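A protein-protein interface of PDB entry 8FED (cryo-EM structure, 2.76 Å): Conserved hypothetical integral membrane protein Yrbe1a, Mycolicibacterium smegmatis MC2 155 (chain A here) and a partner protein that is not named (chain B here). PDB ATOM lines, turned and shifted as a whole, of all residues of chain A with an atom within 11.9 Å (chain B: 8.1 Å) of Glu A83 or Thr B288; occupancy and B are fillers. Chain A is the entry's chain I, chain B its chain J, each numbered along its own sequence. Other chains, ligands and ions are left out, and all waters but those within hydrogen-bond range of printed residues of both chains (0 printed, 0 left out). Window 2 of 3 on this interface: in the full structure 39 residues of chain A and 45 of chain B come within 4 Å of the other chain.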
ATOM      1  N   ILE A  74      -9.736   5.345 -12.150  1.00  0.00           N
ATOM      2  CA  ILE A  74      -8.497   5.924 -11.639  1.00  0.00           C
ATOM      3  C   ILE A  74      -8.158   7.208 -12.383  1.00  0.00           C
ATOM      4  O   ILE A  74      -7.752   8.202 -11.772  1.00  0.00           O
ATOM      5  CB  ILE A  74      -7.352   4.898 -11.722  1.00  0.00           C
ATOM      6  CG1 ILE A  74      -7.601   3.752 -10.745  1.00  0.00           C
ATOM      7  CG2 ILE A  74      -6.014   5.550 -11.431  1.00  0.00           C
ATOM      8  CD1 ILE A  74      -8.056   4.203  -9.395  1.00  0.00           C
ATOM      9  N   PHE A  75      -8.310   7.206 -13.709  1.00  0.00           N
ATOM     10  CA  PHE A  75      -8.020   8.400 -14.495  1.00  0.00           C
ATOM     11  C   PHE A  75      -8.913   9.563 -14.079  1.00  0.00           C
ATOM     12  O   PHE A  75      -8.432  10.686 -13.861  1.00  0.00           O
ATOM     13  CB  PHE A  75      -8.183   8.081 -15.984  1.00  0.00           C
ATOM     14  CG  PHE A  75      -8.214   9.292 -16.872  1.00  0.00           C
ATOM     15  CD1 PHE A  75      -7.039   9.897 -17.280  1.00  0.00           C
ATOM     16  CD2 PHE A  75      -9.418   9.804 -17.327  1.00  0.00           C
ATOM     17  CE1 PHE A  75      -7.066  11.003 -18.102  1.00  0.00           C
ATOM     18  CE2 PHE A  75      -9.448  10.909 -18.149  1.00  0.00           C
ATOM     19  CZ  PHE A  75      -8.271  11.508 -18.539  1.00  0.00           C
ATOM     20  N   THR A  76     -10.219   9.309 -13.957  1.00  0.00           N
ATOM     21  CA  THR A  76     -11.150  10.365 -13.568  1.00  0.00           C
ATOM     22  C   THR A  76     -10.819  10.904 -12.182  1.00  0.00           C
ATOM     23  O   THR A  76     -10.750  12.125 -11.974  1.00  0.00           O
ATOM     24  CB  THR A  76     -12.586   9.840 -13.612  1.00  0.00           C
ATOM     25  OG1 THR A  76     -12.939   9.527 -14.964  1.00  0.00           O
ATOM     26  CG2 THR A  76     -13.553  10.879 -13.073  1.00  0.00           C
ATOM     27  N   LEU A  77     -10.595  10.002 -11.223  1.00  0.00           N
ATOM     28  CA  LEU A  77     -10.284  10.426  -9.862  1.00  0.00           C
ATOM     29  C   LEU A  77      -8.994  11.232  -9.819  1.00  0.00           C
ATOM     30  O   LEU A  77      -8.926  12.271  -9.152  1.00  0.00           O
ATOM     31  CB  LEU A  77     -10.186   9.207  -8.947  1.00  0.00           C
ATOM     32  CG  LEU A  77     -10.043   9.471  -7.450  1.00  0.00           C
ATOM     33  CD1 LEU A  77     -11.299  10.119  -6.893  1.00  0.00           C
ATOM     34  CD2 LEU A  77      -9.730   8.181  -6.716  1.00  0.00           C
ATOM     35  N   ASN A  78      -7.965  10.779 -10.541  1.00  0.00           N
ATOM     36  CA  ASN A  78      -6.681  11.468 -10.523  1.00  0.00           C
ATOM     37  C   ASN A  78      -6.786  12.862 -11.121  1.00  0.00           C
ATOM     38  O   ASN A  78      -6.238  13.816 -10.561  1.00  0.00           O
ATOM     39  CB  ASN A  78      -5.628  10.653 -11.267  1.00  0.00           C
ATOM     40  CG  ASN A  78      -5.131   9.474 -10.467  1.00  0.00           C
ATOM     41  OD1 ASN A  78      -5.314   9.416  -9.254  1.00  0.00           O
ATOM     42  ND2 ASN A  78      -4.487   8.532 -11.140  1.00  0.00           N
ATOM     43  N   ILE A  79      -7.477  13.010 -12.256  1.00  0.00           N
ATOM     44  CA  ILE A  79      -7.549  14.338 -12.863  1.00  0.00           C
ATOM     45  C   ILE A  79      -8.378  15.281 -11.995  1.00  0.00           C
ATOM     46  O   ILE A  79      -7.995  16.443 -11.781  1.00  0.00           O
ATOM     47  CB  ILE A  79      -8.062  14.271 -14.318  1.00  0.00           C
ATOM     48  CG1 ILE A  79      -9.472  13.688 -14.413  1.00  0.00           C
ATOM     49  CG2 ILE A  79      -7.095  13.477 -15.184  1.00  0.00           C
ATOM     50  CD1 ILE A  79     -10.035  13.693 -15.814  1.00  0.00           C
ATOM     51  N   LEU A  80      -9.506  14.800 -11.455  1.00  0.00           N
ATOM     52  CA  LEU A  80     -10.327  15.660 -10.609  1.00  0.00           C
ATOM     53  C   LEU A  80      -9.583  16.070  -9.344  1.00  0.00           C
ATOM     54  O   LEU A  80      -9.683  17.222  -8.906  1.00  0.00           O
ATOM     55  CB  LEU A  80     -11.642  14.964 -10.257  1.00  0.00           C
ATOM     56  CG  LEU A  80     -12.615  14.709 -11.409  1.00  0.00           C
ATOM     57  CD1 LEU A  80     -13.947  14.208 -10.876  1.00  0.00           C
ATOM     58  CD2 LEU A  80     -12.810  15.958 -12.250  1.00  0.00           C
ATOM     59  N   LEU A  81      -8.819  15.150  -8.747  1.00  0.00           N
ATOM     60  CA  LEU A  81      -8.092  15.486  -7.527  1.00  0.00           C
ATOM     61  C   LEU A  81      -6.903  16.395  -7.816  1.00  0.00           C
ATOM     62  O   LEU A  81      -6.592  17.286  -7.018  1.00  0.00           O
ATOM     63  CB  LEU A  81      -7.639  14.214  -6.816  1.00  0.00           C
ATOM     64  CG  LEU A  81      -8.746  13.449  -6.088  1.00  0.00           C
ATOM     65  CD1 LEU A  81      -8.169  12.268  -5.341  1.00  0.00           C
ATOM     66  CD2 LEU A  81      -9.499  14.366  -5.141  1.00  0.00           C
ATOM     67  N   ALA A  82      -6.213  16.177  -8.939  1.00  0.00           N
ATOM     68  CA  ALA A  82      -5.095  17.040  -9.300  1.00  0.00           C
ATOM     69  C   ALA A  82      -5.563  18.468  -9.535  1.00  0.00           C
ATOM     70  O   ALA A  82      -4.891  19.423  -9.128  1.00  0.00           O
ATOM     71  CB  ALA A  82      -4.385  16.493 -10.537  1.00  0.00           C
ATOM     72  N   GLU A  83      -6.712  18.637 -10.194  1.00  0.00           N
ATOM     73  CA  GLU A  83      -7.287  19.975 -10.301  1.00  0.00           C
ATOM     74  C   GLU A  83      -7.741  20.491  -8.939  1.00  0.00           C
ATOM     75  O   GLU A  83      -7.648  21.692  -8.663  1.00  0.00           O
ATOM     76  CB  GLU A  83      -8.438  19.974 -11.302  1.00  0.00           C
ATOM     77  CG  GLU A  83      -7.990  19.715 -12.727  1.00  0.00           C
ATOM     78  CD  GLU A  83      -7.011  20.762 -13.230  1.00  0.00           C
ATOM     79  OE1 GLU A  83      -7.194  21.954 -12.908  1.00  0.00           O
ATOM     80  OE2 GLU A  83      -6.054  20.390 -13.941  1.00  0.00           O
ATOM     81  N   PHE A  84      -8.245  19.597  -8.082  1.00  0.00           N
ATOM     82  CA  PHE A  84      -8.594  19.981  -6.718  1.00  0.00           C
ATOM     83  C   PHE A  84      -7.362  20.443  -5.948  1.00  0.00           C
ATOM     84  O   PHE A  84      -7.418  21.425  -5.201  1.00  0.00           O
ATOM     85  CB  PHE A  84      -9.263  18.800  -6.009  1.00  0.00           C
ATOM     86  CG  PHE A  84     -10.126  19.185  -4.840  1.00  0.00           C
ATOM     87  CD1 PHE A  84      -9.566  19.638  -3.656  1.00  0.00           C
ATOM     88  CD2 PHE A  84     -11.503  19.066  -4.918  1.00  0.00           C
ATOM     89  CE1 PHE A  84     -10.363  19.983  -2.582  1.00  0.00           C
ATOM     90  CE2 PHE A  84     -12.306  19.406  -3.846  1.00  0.00           C
ATOM     91  CZ  PHE A  84     -11.734  19.866  -2.677  1.00  0.00           C
ATOM     92  N   GLY A  85      -6.238  19.743  -6.120  1.00  0.00           N
ATOM     93  CA  GLY A  85      -5.003  20.022  -5.405  1.00  0.00           C
ATOM     94  C   GLY A  85      -4.513  18.863  -4.557  1.00  0.00           C
ATOM     95  O   GLY A  85      -3.312  18.764  -4.289  1.00  0.00           O
ATOM     96  N   ALA A  86      -5.422  17.982  -4.137  1.00  0.00           N
ATOM     97  CA  ALA A  86      -5.081  16.855  -3.269  1.00  0.00           C
ATOM     98  C   ALA A  86      -4.969  15.588  -4.113  1.00  0.00           C
ATOM     99  O   ALA A  86      -5.857  14.737  -4.131  1.00  0.00           O
ATOM    100  CB  ALA A  86      -6.118  16.704  -2.160  1.00  0.00           C
ATOM    101  N   ALA A  87      -3.843  15.461  -4.809  1.00  0.00           N
ATOM    102  CA  ALA A  87      -3.584  14.298  -5.647  1.00  0.00           C
ATOM    103  C   ALA A  87      -2.954  13.138  -4.887  1.00  0.00           C
ATOM    104  O   ALA A  87      -2.843  12.043  -5.446  1.00  0.00           O
ATOM    105  CB  ALA A  87      -2.679  14.684  -6.822  1.00  0.00           C
ATOM    106  N   ASP A  88      -2.539  13.349  -3.638  1.00  0.00           N
ATOM    107  CA  ASP A  88      -1.933  12.290  -2.840  1.00  0.00           C
ATOM    108  C   ASP A  88      -2.956  11.409  -2.137  1.00  0.00           C
ATOM    109  O   ASP A  88      -2.579  10.365  -1.597  1.00  0.00           O
ATOM    110  CB  ASP A  88      -0.982  12.891  -1.804  1.00  0.00           C
ATOM    111  CG  ASP A  88       0.174  13.631  -2.438  1.00  0.00           C
ATOM    112  OD1 ASP A  88       0.568  13.263  -3.564  1.00  0.00           O
ATOM    113  OD2 ASP A  88       0.690  14.581  -1.812  1.00  0.00           O
ATOM    114  N   VAL A  89      -4.226  11.800  -2.129  1.00  0.00           N
ATOM    115  CA  VAL A  89      -5.274  11.022  -1.489  1.00  0.00           C
ATOM    116  C   VAL A  89      -6.085  10.225  -2.512  1.00  0.00           C
ATOM    117  O   VAL A  89      -7.209   9.817  -2.228  1.00  0.00           O
ATOM    118  CB  VAL A  89      -6.183  11.910  -0.629  1.00  0.00           C
ATOM    119  CG1 VAL A  89      -5.385  12.524   0.505  1.00  0.00           C
ATOM    120  CG2 VAL A  89      -6.811  12.995  -1.482  1.00  0.00           C
ATOM    121  N   SER A  90      -5.527  10.001  -3.703  1.00  0.00           N
ATOM    122  CA  SER A  90      -6.226   9.217  -4.716  1.00  0.00           C
ATOM    123  C   SER A  90      -6.322   7.749  -4.328  1.00  0.00           C
ATOM    124  O   SER A  90      -7.285   7.073  -4.709  1.00  0.00           O
ATOM    125  CB  SER A  90      -5.522   9.361  -6.063  1.00  0.00           C
ATOM    126  OG  SER A  90      -4.202   8.852  -6.002  1.00  0.00           O
ATOM    127  N   GLN A 181       0.063   8.865 -15.211  1.00  0.00           N
ATOM    128  CA  GLN A 181      -0.276  10.180 -14.686  1.00  0.00           C
ATOM    129  C   GLN A 181       0.761  10.717 -13.709  1.00  0.00           C
ATOM    130  O   GLN A 181       0.574  11.817 -13.176  1.00  0.00           O
ATOM    131  CB  GLN A 181      -1.651  10.133 -14.018  1.00  0.00           C
ATOM    132  CG  GLN A 181      -2.759   9.717 -14.966  1.00  0.00           C
ATOM    133  CD  GLN A 181      -4.133   9.848 -14.352  1.00  0.00           C
ATOM    134  OE1 GLN A 181      -4.651   8.904 -13.761  1.00  0.00           O
ATOM    135  NE2 GLN A 181      -4.734  11.023 -14.493  1.00  0.00           N
ATOM    136  N   VAL A 183       1.706  10.166 -10.653  1.00  0.00           N
ATOM    137  CA  VAL A 183       1.440  10.396  -9.237  1.00  0.00           C
ATOM    138  C   VAL A 183       2.482   9.629  -8.436  1.00  0.00           C
ATOM    139  O   VAL A 183       3.202   8.786  -8.981  1.00  0.00           O
ATOM    140  CB  VAL A 183       0.011   9.981  -8.841  1.00  0.00           C
ATOM    141  CG1 VAL A 183      -1.007  10.645  -9.750  1.00  0.00           C
ATOM    142  CG2 VAL A 183      -0.136   8.470  -8.866  1.00  0.00           C
ATOM    143  N   PHE B 214     -20.620  23.246 -11.241  1.00  0.00           N
ATOM    144  CA  PHE B 214     -19.514  22.415 -11.699  1.00  0.00           C
ATOM    145  C   PHE B 214     -19.906  21.454 -12.814  1.00  0.00           C
ATOM    146  O   PHE B 214     -19.106  20.588 -13.180  1.00  0.00           O
ATOM    147  CB  PHE B 214     -18.922  21.640 -10.520  1.00  0.00           C
ATOM    148  CG  PHE B 214     -18.308  22.518  -9.469  1.00  0.00           C
ATOM    149  CD1 PHE B 214     -16.980  22.895  -9.554  1.00  0.00           C
ATOM    150  CD2 PHE B 214     -19.059  22.972  -8.399  1.00  0.00           C
ATOM    151  CE1 PHE B 214     -16.413  23.705  -8.594  1.00  0.00           C
ATOM    152  CE2 PHE B 214     -18.495  23.784  -7.435  1.00  0.00           C
ATOM    153  CZ  PHE B 214     -17.171  24.148  -7.534  1.00  0.00           C
ATOM    154  N   THR B 281      -5.881  15.812 -22.002  1.00  0.00           N
ATOM    155  CA  THR B 281      -5.052  16.997 -21.814  1.00  0.00           C
ATOM    156  C   THR B 281      -5.769  18.089 -21.030  1.00  0.00           C
ATOM    157  O   THR B 281      -5.203  18.647 -20.085  1.00  0.00           O
ATOM    158  CB  THR B 281      -4.597  17.540 -23.174  1.00  0.00           C
ATOM    159  OG1 THR B 281      -3.869  16.524 -23.875  1.00  0.00           O
ATOM    160  CG2 THR B 281      -3.704  18.757 -22.994  1.00  0.00           C
ATOM    161  N   ASP B 282      -7.009  18.404 -21.399  1.00  0.00           N
ATOM    162  CA  ASP B 282      -7.769  19.435 -20.712  1.00  0.00           C
ATOM    163  C   ASP B 282      -8.815  18.773 -19.831  1.00  0.00           C
ATOM    164  O   ASP B 282      -9.795  18.224 -20.356  1.00  0.00           O
ATOM    165  CB  ASP B 282      -8.434  20.372 -21.719  1.00  0.00           C
ATOM    166  CG  ASP B 282      -9.057  21.590 -21.064  1.00  0.00           C
ATOM    167  OD1 ASP B 282      -8.847  21.795 -19.851  1.00  0.00           O
ATOM    168  OD2 ASP B 282      -9.762  22.345 -21.767  1.00  0.00           O
ATOM    169  N   PRO B 283      -8.658  18.791 -18.504  1.00  0.00           N
ATOM    170  CA  PRO B 283      -9.620  18.093 -17.637  1.00  0.00           C
ATOM    171  C   PRO B 283     -11.013  18.696 -17.643  1.00  0.00           C
ATOM    172  O   PRO B 283     -11.954  18.017 -17.213  1.00  0.00           O
ATOM    173  CB  PRO B 283      -8.978  18.195 -16.248  1.00  0.00           C
ATOM    174  CG  PRO B 283      -8.109  19.398 -16.331  1.00  0.00           C
ATOM    175  CD  PRO B 283      -7.580  19.429 -17.732  1.00  0.00           C
ATOM    176  N   ASN B 284     -11.167  19.940 -18.104  1.00  0.00           N
ATOM    177  CA  ASN B 284     -12.456  20.638 -18.140  1.00  0.00           C
ATOM    178  C   ASN B 284     -13.076  20.716 -16.744  1.00  0.00           C
ATOM    179  O   ASN B 284     -14.224  20.327 -16.523  1.00  0.00           O
ATOM    180  CB  ASN B 284     -13.414  19.980 -19.138  1.00  0.00           C
ATOM    181  CG  ASN B 284     -14.601  20.859 -19.476  1.00  0.00           C
ATOM    182  OD1 ASN B 284     -14.498  22.084 -19.482  1.00  0.00           O
ATOM    183  ND2 ASN B 284     -15.740  20.236 -19.753  1.00  0.00           N
ATOM    184  N   PHE B 285     -12.294  21.227 -15.795  1.00  0.00           N
ATOM    185  CA  PHE B 285     -12.740  21.361 -14.413  1.00  0.00           C
ATOM    186  C   PHE B 285     -11.799  22.305 -13.680  1.00  0.00           C
ATOM    187  O   PHE B 285     -10.585  22.086 -13.674  1.00  0.00           O
ATOM    188  CB  PHE B 285     -12.790  19.997 -13.716  1.00  0.00           C
ATOM    189  CG  PHE B 285     -12.961  20.085 -12.233  1.00  0.00           C
ATOM    190  CD1 PHE B 285     -14.155  20.514 -11.688  1.00  0.00           C
ATOM    191  CD2 PHE B 285     -11.932  19.727 -11.384  1.00  0.00           C
ATOM    192  CE1 PHE B 285     -14.312  20.598 -10.326  1.00  0.00           C
ATOM    193  CE2 PHE B 285     -12.085  19.806 -10.017  1.00  0.00           C
ATOM    194  CZ  PHE B 285     -13.275  20.242  -9.488  1.00  0.00           C
ATOM    195  N   ASN B 286     -12.360  23.347 -13.066  1.00  0.00           N
ATOM    196  CA  ASN B 286     -11.587  24.346 -12.338  1.00  0.00           C
ATOM    197  C   ASN B 286     -12.192  24.558 -10.959  1.00  0.00           C
ATOM    198  O   ASN B 286     -13.389  24.836 -10.840  1.00  0.00           O
ATOM    199  CB  ASN B 286     -11.547  25.678 -13.096  1.00  0.00           C
ATOM    200  CG  ASN B 286     -10.865  25.564 -14.442  1.00  0.00           C
ATOM    201  OD1 ASN B 286     -11.485  25.187 -15.435  1.00  0.00           O
ATOM    202  ND2 ASN B 286      -9.583  25.901 -14.484  1.00  0.00           N
ATOM    203  N   LEU B 287     -11.371  24.406  -9.922  1.00  0.00           N
ATOM    204  CA  LEU B 287     -11.743  24.786  -8.564  1.00  0.00           C
ATOM    205  C   LEU B 287     -10.796  25.811  -7.960  1.00  0.00           C
ATOM    206  O   LEU B 287     -11.251  26.802  -7.378  1.00  0.00           O
ATOM    207  CB  LEU B 287     -11.810  23.547  -7.658  1.00  0.00           C
ATOM    208  CG  LEU B 287     -12.271  23.835  -6.228  1.00  0.00           C
ATOM    209  CD1 LEU B 287     -13.705  24.334  -6.219  1.00  0.00           C
ATOM    210  CD2 LEU B 287     -12.128  22.608  -5.356  1.00  0.00           C
ATOM    211  N   THR B 288      -9.487  25.601  -8.079  1.00  0.00           N
ATOM    212  CA  THR B 288      -8.498  26.473  -7.466  1.00  0.00           C
ATOM    213  C   THR B 288      -8.091  27.570  -8.451  1.00  0.00           C
ATOM    214  O   THR B 288      -8.711  27.753  -9.501  1.00  0.00           O
ATOM    215  CB  THR B 288      -7.296  25.656  -6.997  1.00  0.00           C
ATOM    216  OG1 THR B 288      -6.331  26.525  -6.392  1.00  0.00           O
ATOM    217  CG2 THR B 288      -6.652  24.932  -8.168  1.00  0.00           C
ATOM    218  N   VAL B 289      -7.037  28.310  -8.121  1.00  0.00           N
ATOM    219  CA  VAL B 289      -6.598  29.417  -8.961  1.00  0.00           C
ATOM    220  C   VAL B 289      -5.645  28.911 -10.038  1.00  0.00           C
ATOM    221  O   VAL B 289      -5.315  29.632 -10.980  1.00  0.00           O
ATOM    222  CB  VAL B 289      -5.922  30.524  -8.126  1.00  0.00           C
ATOM    223  CG1 VAL B 289      -6.907  31.143  -7.147  1.00  0.00           C
ATOM    224  CG2 VAL B 289      -4.702  30.001  -7.420  1.00  0.00           C
ATOM    225  OXT VAL B 289      -5.177  27.774  -9.993  1.00  0.00           O
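The side-chain carboxylate (OE1) of Glu A83 sits close to the backbone carbonyl oxygen (O) of Phe B285 (3.5 Å).
Among the printed residues, pairs that only touch across the chains: Leu A80 with Phe B285 (3.7 Å), Glu A83 with Pro B283 (3.3 Å), Glu A83 with Thr B288 (3.4 Å) and Phe A84 with Leu B287 (3.5 Å).
Printed residues of chain A that touch a printed residue of chain B: Leu A80, Glu A83 and Phe A84.
Along chain A the printed residues that touch a printed residue of chain B span positions 80 to 84.
Among the printed residues, 5 pairs touch across the chains.
Among the printed residues, no Asp or Glu carboxylate lies within 4 Å of a Lys or Arg side-chain nitrogen of the other chain.
Phe A75 touches none of the printed residues of chain B.
Of the printed residues of chain B, Leu A80 touches Phe B285.
Of chain B, only Pro B283, Phe B285 and Thr B288 come within 4 Å of Glu A83.
Of the printed residues of chain B, Phe A84 touches Leu B287 (3.5 Å).
Of chain A, only Glu A83 comes within 4 Å of Pro B283.
No residue of chain A comes within 4 Å of Asn B286.
Leu B287 touches one residue of chain A.
Of chain A, only Glu A83 comes within 4 Å of Thr B288.
No residue of chain A comes within 4 Å of Val B289.
The nearest printed residue of chain B that does not touch Leu A80 is Pro B283 (5.4 Å).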
